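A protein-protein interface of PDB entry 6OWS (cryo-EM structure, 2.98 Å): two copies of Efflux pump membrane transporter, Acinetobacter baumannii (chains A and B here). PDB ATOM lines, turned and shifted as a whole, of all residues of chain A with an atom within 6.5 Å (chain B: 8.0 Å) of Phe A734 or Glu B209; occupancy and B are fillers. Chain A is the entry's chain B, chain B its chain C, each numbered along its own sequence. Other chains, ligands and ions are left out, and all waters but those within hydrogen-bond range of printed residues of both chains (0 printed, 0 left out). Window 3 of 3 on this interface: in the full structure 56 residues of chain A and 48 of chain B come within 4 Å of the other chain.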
ATOM      1  N   ILE A 722      19.934   3.070  13.012  1.00  0.00           N
ATOM      2  CA  ILE A 722      20.608   2.086  13.847  1.00  0.00           C
ATOM      3  C   ILE A 722      21.863   1.609  13.138  1.00  0.00           C
ATOM      4  O   ILE A 722      21.827   1.257  11.955  1.00  0.00           O
ATOM      5  CB  ILE A 722      19.671   0.922  14.172  1.00  0.00           C
ATOM      6  CG1 ILE A 722      18.297   1.463  14.549  1.00  0.00           C
ATOM      7  CG2 ILE A 722      20.228   0.114  15.305  1.00  0.00           C
ATOM      8  CD1 ILE A 722      17.279   0.400  14.821  1.00  0.00           C
ATOM      9  N   ARG A 724      23.991  -1.085  12.742  1.00  0.00           N
ATOM     10  CA  ARG A 724      24.023  -2.512  12.872  1.00  0.00           C
ATOM     11  C   ARG A 724      25.325  -3.183  13.002  1.00  0.00           C
ATOM     12  O   ARG A 724      25.435  -4.154  13.685  1.00  0.00           O
ATOM     13  CB  ARG A 724      23.296  -3.107  11.729  1.00  0.00           C
ATOM     14  CG  ARG A 724      21.834  -2.907  11.846  1.00  0.00           C
ATOM     15  CD  ARG A 724      21.253  -3.474  10.627  1.00  0.00           C
ATOM     16  NE  ARG A 724      20.057  -4.211  10.857  1.00  0.00           N
ATOM     17  CZ  ARG A 724      18.898  -3.707  10.588  1.00  0.00           C
ATOM     18  NH1 ARG A 724      17.815  -4.393  10.755  1.00  0.00           N
ATOM     19  NH2 ARG A 724      18.847  -2.488  10.154  1.00  0.00           N
ATOM     20  N   LEU A 727      26.399  -2.887  16.291  1.00  0.00           N
ATOM     21  CA  LEU A 727      25.468  -3.603  17.146  1.00  0.00           C
ATOM     22  C   LEU A 727      25.790  -5.085  17.223  1.00  0.00           C
ATOM     23  O   LEU A 727      25.481  -5.728  18.229  1.00  0.00           O
ATOM     24  CB  LEU A 727      24.046  -3.404  16.642  1.00  0.00           C
ATOM     25  CG  LEU A 727      22.943  -3.440  17.682  1.00  0.00           C
ATOM     26  CD1 LEU A 727      23.304  -2.605  18.878  1.00  0.00           C
ATOM     27  CD2 LEU A 727      21.691  -2.921  17.054  1.00  0.00           C
ATOM     28  N   VAL A 732      25.238  -7.522  20.964  1.00  0.00           N
ATOM     29  CA  VAL A 732      23.873  -7.097  21.230  1.00  0.00           C
ATOM     30  C   VAL A 732      22.976  -7.672  20.154  1.00  0.00           C
ATOM     31  O   VAL A 732      23.187  -7.430  18.962  1.00  0.00           O
ATOM     32  CB  VAL A 732      23.767  -5.571  21.275  1.00  0.00           C
ATOM     33  CG1 VAL A 732      22.373  -5.174  21.668  1.00  0.00           C
ATOM     34  CG2 VAL A 732      24.769  -5.017  22.248  1.00  0.00           C
ATOM     35  N   LYS A 733      21.993  -8.454  20.570  1.00  0.00           N
ATOM     36  CA  LYS A 733      20.994  -8.965  19.650  1.00  0.00           C
ATOM     37  C   LYS A 733      20.152  -7.811  19.130  1.00  0.00           C
ATOM     38  O   LYS A 733      19.767  -6.922  19.890  1.00  0.00           O
ATOM     39  CB  LYS A 733      20.128  -9.995  20.370  1.00  0.00           C
ATOM     40  CG  LYS A 733      19.133 -10.723  19.511  1.00  0.00           C
ATOM     41  CD  LYS A 733      18.488 -11.851  20.300  1.00  0.00           C
ATOM     42  CE  LYS A 733      17.409 -12.549  19.495  1.00  0.00           C
ATOM     43  NZ  LYS A 733      17.970 -13.205  18.285  1.00  0.00           N
ATOM     44  N   PHE A 734      19.899  -7.802  17.817  1.00  0.00           N
ATOM     45  CA  PHE A 734      19.096  -6.735  17.230  1.00  0.00           C
ATOM     46  C   PHE A 734      17.657  -6.774  17.702  1.00  0.00           C
ATOM     47  O   PHE A 734      16.995  -5.734  17.706  1.00  0.00           O
ATOM     48  CB  PHE A 734      19.125  -6.806  15.704  1.00  0.00           C
ATOM     49  CG  PHE A 734      18.502  -5.619  15.036  1.00  0.00           C
ATOM     50  CD1 PHE A 734      19.208  -4.446  14.901  1.00  0.00           C
ATOM     51  CD2 PHE A 734      17.214  -5.672  14.546  1.00  0.00           C
ATOM     52  CE1 PHE A 734      18.644  -3.350  14.295  1.00  0.00           C
ATOM     53  CE2 PHE A 734      16.648  -4.577  13.943  1.00  0.00           C
ATOM     54  CZ  PHE A 734      17.364  -3.418  13.820  1.00  0.00           C
ATOM     55  N   SER A 735      17.167  -7.945  18.106  1.00  0.00           N
ATOM     56  CA  SER A 735      15.799  -8.060  18.585  1.00  0.00           C
ATOM     57  C   SER A 735      15.585  -7.287  19.875  1.00  0.00           C
ATOM     58  O   SER A 735      14.494  -6.766  20.099  1.00  0.00           O
ATOM     59  CB  SER A 735      15.446  -9.523  18.798  1.00  0.00           C
ATOM     60  OG  SER A 735      14.922 -10.104  17.627  1.00  0.00           O
ATOM     61  N   ASP A 736      16.602  -7.182  20.721  1.00  0.00           N
ATOM     62  CA  ASP A 736      16.419  -6.462  21.968  1.00  0.00           C
ATOM     63  C   ASP A 736      16.589  -4.963  21.826  1.00  0.00           C
ATOM     64  O   ASP A 736      16.167  -4.223  22.716  1.00  0.00           O
ATOM     65  CB  ASP A 736      17.378  -6.981  23.036  1.00  0.00           C
ATOM     66  CG  ASP A 736      16.994  -8.357  23.538  1.00  0.00           C
ATOM     67  OD1 ASP A 736      16.203  -9.044  22.862  1.00  0.00           O
ATOM     68  OD2 ASP A 736      17.462  -8.735  24.632  1.00  0.00           O
ATOM     69  N   VAL A 737      17.202  -4.495  20.747  1.00  0.00           N
ATOM     70  CA  VAL A 737      17.260  -3.061  20.500  1.00  0.00           C
ATOM     71  C   VAL A 737      15.945  -2.583  19.911  1.00  0.00           C
ATOM     72  O   VAL A 737      15.425  -1.526  20.282  1.00  0.00           O
ATOM     73  CB  VAL A 737      18.465  -2.745  19.590  1.00  0.00           C
ATOM     74  CG1 VAL A 737      18.322  -1.416  18.893  1.00  0.00           C
ATOM     75  CG2 VAL A 737      19.740  -2.753  20.395  1.00  0.00           C
ATOM     76  N   SER A 738      15.345  -3.392  19.049  1.00  0.00           N
ATOM     77  CA  SER A 738      14.164  -2.979  18.311  1.00  0.00           C
ATOM     78  C   SER A 738      12.886  -3.019  19.126  1.00  0.00           C
ATOM     79  O   SER A 738      11.849  -2.605  18.608  1.00  0.00           O
ATOM     80  CB  SER A 738      13.983  -3.855  17.082  1.00  0.00           C
ATOM     81  OG  SER A 738      12.985  -4.831  17.313  1.00  0.00           O
ATOM     82  N   ASP A 739      12.902  -3.525  20.356  1.00  0.00           N
ATOM     83  CA  ASP A 739      11.698  -3.479  21.169  1.00  0.00           C
ATOM     84  C   ASP A 739      11.865  -2.701  22.461  1.00  0.00           C
ATOM     85  O   ASP A 739      10.882  -2.507  23.175  1.00  0.00           O
ATOM     86  CB  ASP A 739      11.192  -4.891  21.482  1.00  0.00           C
ATOM     87  CG  ASP A 739      12.268  -5.800  21.996  1.00  0.00           C
ATOM     88  OD1 ASP A 739      13.361  -5.314  22.336  1.00  0.00           O
ATOM     89  OD2 ASP A 739      12.027  -7.023  22.054  1.00  0.00           O
ATOM     90  N   ASP B 202      14.527 -21.633  10.401  1.00  0.00           N
ATOM     91  CA  ASP B 202      15.562 -20.781  10.960  1.00  0.00           C
ATOM     92  C   ASP B 202      15.950 -19.661  10.015  1.00  0.00           C
ATOM     93  O   ASP B 202      16.366 -18.594  10.472  1.00  0.00           O
ATOM     94  CB  ASP B 202      16.796 -21.611  11.307  1.00  0.00           C
ATOM     95  CG  ASP B 202      16.600 -22.458  12.548  1.00  0.00           C
ATOM     96  OD1 ASP B 202      16.107 -21.927  13.565  1.00  0.00           O
ATOM     97  OD2 ASP B 202      16.937 -23.658  12.512  1.00  0.00           O
ATOM     98  N   VAL B 203      15.830 -19.885   8.709  1.00  0.00           N
ATOM     99  CA  VAL B 203      16.022 -18.806   7.749  1.00  0.00           C
ATOM    100  C   VAL B 203      14.860 -17.831   7.825  1.00  0.00           C
ATOM    101  O   VAL B 203      15.040 -16.618   7.691  1.00  0.00           O
ATOM    102  CB  VAL B 203      16.196 -19.388   6.335  1.00  0.00           C
ATOM    103  CG1 VAL B 203      16.385 -18.301   5.308  1.00  0.00           C
ATOM    104  CG2 VAL B 203      17.375 -20.327   6.303  1.00  0.00           C
ATOM    105  N   ASN B 204      13.657 -18.341   8.079  1.00  0.00           N
ATOM    106  CA  ASN B 204      12.492 -17.478   8.220  1.00  0.00           C
ATOM    107  C   ASN B 204      12.579 -16.624   9.470  1.00  0.00           C
ATOM    108  O   ASN B 204      12.207 -15.449   9.449  1.00  0.00           O
ATOM    109  CB  ASN B 204      11.222 -18.314   8.259  1.00  0.00           C
ATOM    110  CG  ASN B 204      10.864 -18.880   6.923  1.00  0.00           C
ATOM    111  OD1 ASN B 204      11.506 -18.584   5.925  1.00  0.00           O
ATOM    112  ND2 ASN B 204       9.827 -19.695   6.885  1.00  0.00           N
ATOM    113  N   ASN B 205      13.063 -17.192  10.570  1.00  0.00           N
ATOM    114  CA  ASN B 205      13.125 -16.442  11.816  1.00  0.00           C
ATOM    115  C   ASN B 205      14.241 -15.414  11.819  1.00  0.00           C
ATOM    116  O   ASN B 205      14.155 -14.424  12.549  1.00  0.00           O
ATOM    117  CB  ASN B 205      13.304 -17.389  12.993  1.00  0.00           C
ATOM    118  CG  ASN B 205      12.034 -18.105  13.352  1.00  0.00           C
ATOM    119  OD1 ASN B 205      12.059 -19.111  14.052  1.00  0.00           O
ATOM    120  ND2 ASN B 205      10.909 -17.596  12.873  1.00  0.00           N
ATOM    121  N   ALA B 206      15.290 -15.626  11.031  1.00  0.00           N
ATOM    122  CA  ALA B 206      16.364 -14.646  10.974  1.00  0.00           C
ATOM    123  C   ALA B 206      15.939 -13.399  10.229  1.00  0.00           C
ATOM    124  O   ALA B 206      16.413 -12.304  10.538  1.00  0.00           O
ATOM    125  CB  ALA B 206      17.590 -15.248  10.311  1.00  0.00           C
ATOM    126  N   ILE B 207      15.062 -13.546   9.242  1.00  0.00           N
ATOM    127  CA  ILE B 207      14.593 -12.384   8.510  1.00  0.00           C
ATOM    128  C   ILE B 207      13.624 -11.588   9.362  1.00  0.00           C
ATOM    129  O   ILE B 207      13.611 -10.356   9.310  1.00  0.00           O
ATOM    130  CB  ILE B 207      13.977 -12.832   7.177  1.00  0.00           C
ATOM    131  CG1 ILE B 207      15.019 -13.591   6.368  1.00  0.00           C
ATOM    132  CG2 ILE B 207      13.497 -11.660   6.370  1.00  0.00           C
ATOM    133  CD1 ILE B 207      14.481 -14.199   5.118  1.00  0.00           C
ATOM    134  N   ARG B 208      12.840 -12.267  10.199  1.00  0.00           N
ATOM    135  CA  ARG B 208      11.863 -11.569  11.025  1.00  0.00           C
ATOM    136  C   ARG B 208      12.524 -10.765  12.132  1.00  0.00           C
ATOM    137  O   ARG B 208      11.984  -9.738  12.551  1.00  0.00           O
ATOM    138  CB  ARG B 208      10.876 -12.567  11.614  1.00  0.00           C
ATOM    139  CG  ARG B 208       9.963 -13.175  10.592  1.00  0.00           C
ATOM    140  CD  ARG B 208       8.807 -13.886  11.239  1.00  0.00           C
ATOM    141  NE  ARG B 208       7.975 -14.559  10.251  1.00  0.00           N
ATOM    142  CZ  ARG B 208       7.944 -15.872  10.073  1.00  0.00           C
ATOM    143  NH1 ARG B 208       7.156 -16.396   9.149  1.00  0.00           N
ATOM    144  NH2 ARG B 208       8.695 -16.665  10.820  1.00  0.00           N
ATOM    145  N   GLU B 209      13.683 -11.201  12.613  1.00  0.00           N
ATOM    146  CA  GLU B 209      14.388 -10.426  13.621  1.00  0.00           C
ATOM    147  C   GLU B 209      15.090  -9.224  13.014  1.00  0.00           C
ATOM    148  O   GLU B 209      15.124  -8.153  13.621  1.00  0.00           O
ATOM    149  CB  GLU B 209      15.412 -11.297  14.335  1.00  0.00           C
ATOM    150  CG  GLU B 209      14.824 -12.432  15.124  1.00  0.00           C
ATOM    151  CD  GLU B 209      15.887 -13.376  15.639  1.00  0.00           C
ATOM    152  OE1 GLU B 209      17.077 -13.009  15.593  1.00  0.00           O
ATOM    153  OE2 GLU B 209      15.534 -14.487  16.085  1.00  0.00           O
ATOM    154  N   ASN B 210      15.638  -9.377  11.817  1.00  0.00           N
ATOM    155  CA  ASN B 210      16.544  -8.390  11.258  1.00  0.00           C
ATOM    156  C   ASN B 210      15.875  -7.439  10.285  1.00  0.00           C
ATOM    157  O   ASN B 210      16.490  -6.443   9.901  1.00  0.00           O
ATOM    158  CB  ASN B 210      17.696  -9.091  10.552  1.00  0.00           C
ATOM    159  CG  ASN B 210      18.686  -9.677  11.512  1.00  0.00           C
ATOM    160  OD1 ASN B 210      19.772  -9.137  11.700  1.00  0.00           O
ATOM    161  ND2 ASN B 210      18.325 -10.789  12.129  1.00  0.00           N
ATOM    162  N   ASN B 211      14.649  -7.711   9.881  1.00  0.00           N
ATOM    163  CA  ASN B 211      13.888  -6.819   9.015  1.00  0.00           C
ATOM    164  C   ASN B 211      12.588  -6.568   9.755  1.00  0.00           C
ATOM    165  O   ASN B 211      11.576  -7.212   9.495  1.00  0.00           O
ATOM    166  CB  ASN B 211      13.662  -7.444   7.674  1.00  0.00           C
ATOM    167  CG  ASN B 211      13.002  -6.513   6.709  1.00  0.00           C
ATOM    168  OD1 ASN B 211      13.431  -5.384   6.540  1.00  0.00           O
ATOM    169  ND2 ASN B 211      11.942  -6.974   6.074  1.00  0.00           N
ATOM    170  N   VAL B 212      12.612  -5.608  10.669  1.00  0.00           N
ATOM    171  CA  VAL B 212      11.538  -5.444  11.629  1.00  0.00           C
ATOM    172  C   VAL B 212      10.997  -4.026  11.506  1.00  0.00           C
ATOM    173  O   VAL B 212      11.675  -3.111  11.038  1.00  0.00           O
ATOM    174  CB  VAL B 212      12.023  -5.766  13.062  1.00  0.00           C
ATOM    175  CG1 VAL B 212      12.864  -4.655  13.625  1.00  0.00           C
ATOM    176  CG2 VAL B 212      10.869  -6.125  13.993  1.00  0.00           C
ATOM    177  N   GLU B 213       9.735  -3.869  11.878  1.00  0.00           N
ATOM    178  CA  GLU B 213       9.042  -2.593  11.816  1.00  0.00           C
ATOM    179  C   GLU B 213       8.874  -2.070  13.236  1.00  0.00           C
ATOM    180  O   GLU B 213       8.159  -2.668  14.044  1.00  0.00           O
ATOM    181  CB  GLU B 213       7.697  -2.769  11.123  1.00  0.00           C
ATOM    182  CG  GLU B 213       6.975  -1.487  10.831  1.00  0.00           C
ATOM    183  CD  GLU B 213       5.596  -1.733  10.272  1.00  0.00           C
ATOM    184  OE1 GLU B 213       5.180  -2.909  10.221  1.00  0.00           O
ATOM    185  OE2 GLU B 213       4.927  -0.755   9.881  1.00  0.00           O
ATOM    186  N   ILE B 214       9.533  -0.962  13.540  1.00  0.00           N
ATOM    187  CA  ILE B 214       9.511  -0.380  14.875  1.00  0.00           C
ATOM    188  C   ILE B 214       8.386   0.642  14.951  1.00  0.00           C
ATOM    189  O   ILE B 214       8.226   1.467  14.046  1.00  0.00           O
ATOM    190  CB  ILE B 214      10.869   0.256  15.204  1.00  0.00           C
ATOM    191  CG1 ILE B 214      11.977  -0.766  14.997  1.00  0.00           C
ATOM    192  CG2 ILE B 214      10.904   0.758  16.617  1.00  0.00           C
ATOM    193  CD1 ILE B 214      13.345  -0.233  15.267  1.00  0.00           C
ATOM    194  N   GLN B 237      14.405   3.607  11.837  1.00  0.00           N
ATOM    195  CA  GLN B 237      14.431   2.786  10.634  1.00  0.00           C
ATOM    196  C   GLN B 237      14.901   1.389  10.998  1.00  0.00           C
ATOM    197  O   GLN B 237      16.086   1.175  11.257  1.00  0.00           O
ATOM    198  CB  GLN B 237      15.343   3.401   9.583  1.00  0.00           C
ATOM    199  CG  GLN B 237      15.383   2.610   8.300  1.00  0.00           C
ATOM    200  CD  GLN B 237      14.027   2.500   7.654  1.00  0.00           C
ATOM    201  OE1 GLN B 237      13.509   3.470   7.111  1.00  0.00           O
ATOM    202  NE2 GLN B 237      13.439   1.318   7.711  1.00  0.00           N
ATOM    203  N   GLY B 238      13.980   0.434  11.005  1.00  0.00           N
ATOM    204  CA  GLY B 238      14.326  -0.914  11.396  1.00  0.00           C
ATOM    205  C   GLY B 238      14.526  -1.854  10.232  1.00  0.00           C
ATOM    206  O   GLY B 238      15.215  -2.867  10.358  1.00  0.00           O
ATOM    207  N   GLN B 239      13.947  -1.526   9.087  1.00  0.00           N
ATOM    208  CA  GLN B 239      13.936  -2.451   7.973  1.00  0.00           C
ATOM    209  C   GLN B 239      15.227  -2.361   7.166  1.00  0.00           C
ATOM    210  O   GLN B 239      16.104  -1.538   7.429  1.00  0.00           O
ATOM    211  CB  GLN B 239      12.727  -2.182   7.091  1.00  0.00           C
ATOM    212  CG  GLN B 239      11.447  -2.647   7.725  1.00  0.00           C
ATOM    213  CD  GLN B 239      10.240  -2.012   7.116  1.00  0.00           C
ATOM    214  OE1 GLN B 239      10.334  -0.971   6.483  1.00  0.00           O
ATOM    215  NE2 GLN B 239       9.087  -2.632   7.305  1.00  0.00           N
ATOM    216  N   LEU B 240      15.343  -3.241   6.180  1.00  0.00           N
ATOM    217  CA  LEU B 240      16.477  -3.286   5.275  1.00  0.00           C
ATOM    218  C   LEU B 240      16.057  -2.769   3.907  1.00  0.00           C
ATOM    219  O   LEU B 240      14.875  -2.747   3.569  1.00  0.00           O
ATOM    220  CB  LEU B 240      17.024  -4.707   5.158  1.00  0.00           C
ATOM    221  CG  LEU B 240      17.476  -5.318   6.472  1.00  0.00           C
ATOM    222  CD1 LEU B 240      17.875  -6.749   6.277  1.00  0.00           C
ATOM    223  CD2 LEU B 240      18.631  -4.532   6.994  1.00  0.00           C
ATOM    224  N   ILE B 249      22.594 -11.014   6.884  1.00  0.00           N
ATOM    225  CA  ILE B 249      21.822 -11.433   8.043  1.00  0.00           C
ATOM    226  C   ILE B 249      22.488 -12.660   8.641  1.00  0.00           C
ATOM    227  O   ILE B 249      22.613 -13.696   7.981  1.00  0.00           O
ATOM    228  CB  ILE B 249      20.374 -11.729   7.653  1.00  0.00           C
ATOM    229  CG1 ILE B 249      19.708 -10.470   7.118  1.00  0.00           C
ATOM    230  CG2 ILE B 249      19.626 -12.268   8.831  1.00  0.00           C
ATOM    231  CD1 ILE B 249      18.293 -10.681   6.703  1.00  0.00           C
ATOM    232  N   SER B 250      22.927 -12.550   9.886  1.00  0.00           N
ATOM    233  CA  SER B 250      23.754 -13.591  10.474  1.00  0.00           C
ATOM    234  C   SER B 250      22.909 -14.743  10.994  1.00  0.00           C
ATOM    235  O   SER B 250      21.900 -14.542  11.671  1.00  0.00           O
ATOM    236  CB  SER B 250      24.606 -13.018  11.602  1.00  0.00           C
ATOM    237  OG  SER B 250      25.530 -12.070  11.099  1.00  0.00           O
ATOM    238  N   ILE B 750       7.315 -13.758   4.000  1.00  0.00           N
ATOM    239  CA  ILE B 750       7.765 -13.504   5.363  1.00  0.00           C
ATOM    240  C   ILE B 750       7.251 -12.168   5.873  1.00  0.00           C
ATOM    241  O   ILE B 750       6.411 -12.126   6.776  1.00  0.00           O
ATOM    242  CB  ILE B 750       9.297 -13.555   5.432  1.00  0.00           C
ATOM    243  CG1 ILE B 750       9.806 -14.837   4.796  1.00  0.00           C
ATOM    244  CG2 ILE B 750       9.756 -13.487   6.848  1.00  0.00           C
ATOM    245  CD1 ILE B 750       9.294 -16.076   5.449  1.00  0.00           C
ATOM    246  N   ASN B 751       7.715 -11.077   5.276  1.00  0.00           N
ATOM    247  CA  ASN B 751       7.294  -9.729   5.638  1.00  0.00           C
ATOM    248  C   ASN B 751       7.676  -8.804   4.495  1.00  0.00           C
ATOM    249  O   ASN B 751       8.064  -9.257   3.416  1.00  0.00           O
ATOM    250  CB  ASN B 751       7.917  -9.272   6.956  1.00  0.00           C
ATOM    251  CG  ASN B 751       9.388  -9.520   7.010  1.00  0.00           C
ATOM    252  OD1 ASN B 751       9.944 -10.187   6.151  1.00  0.00           O
ATOM    253  ND2 ASN B 751      10.037  -8.982   8.023  1.00  0.00           N
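No position is printed for both chains.
The side-chain amide nitrogen (ND2) of Asn B210 sits at hydrogen-bond distance from the backbone carbonyl oxygen (O) of Ala B206, 2.9 Å away.
The side-chain amide oxygen (OD1) of Asn B211 lies within hydrogen-bond range of the backbone NH (N) of Leu B240 (2.9 Å).
O of Val B212 sits close to N of Gln B239.
The backbone NH (N) of Gln B239 sits close to the side-chain amide nitrogen (NE2) of Gln B237 (3.2 Å).
The guanidinium group (NH1) of Arg A724 lies within hydrogen-bond range of the backbone carbonyl oxygen (O) of Asn B210, 2.6 Å away.
The guanidinium group (NH1) of Arg A724 sits at hydrogen-bond distance from the backbone carbonyl oxygen (O) of Gly B238 (3.0 Å).
The side-chain carboxylate (OE1) of Glu B209 is in salt-bridge range of the side-chain amino group (NZ) of Lys A733, at 2.8 Å.
Of the 21 printed residues of chain B, 7 touch a printed residue of chain A.
Hydrophobic or aromatic side chains of chain B that line the printed part of chain A: Val B212 and Leu B240.
Of the 11 printed residues of chain A, 6 touch a printed residue of chain B.
Among the printed residues, 10 pairs touch across the chains.
Among the printed residues, merely in contact across the chains: Ile A722 with Gln B237, Arg A724 with Gln B239, Arg A724 with Leu B240, Phe A734 with Glu B209, Phe A734 with Val B212, Ser A735 with Glu B209 and Ser A738 with Val B212.
Printed residues of chain B within 4 Å of Ile A722: Gln B237 (3.8 Å).
Of the printed residues of chain B, Lys A733 touches Glu B209 (2.8 Å).
Ser A735 touches just one residue of chain B: Glu B209.
Asn B204 touches none of the printed residues of chain A.
Glu B209 touches just these residues of chain A: Lys A733 (2.8 Å), Phe A734 (3.4 Å) and Ser A735 (3.4 Å).
Printed residues of chain A within 4 Å of Val B212: Phe A734 and Ser A738.
Printed residues of chain A within 4 Å of Gly B238: Arg A724.
Printed residues of chain A within 4 Å of Leu B240: Arg A724.
The nearest residue of chain B that does not touch Phe A734 is Gly B238 (4.1 Å).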
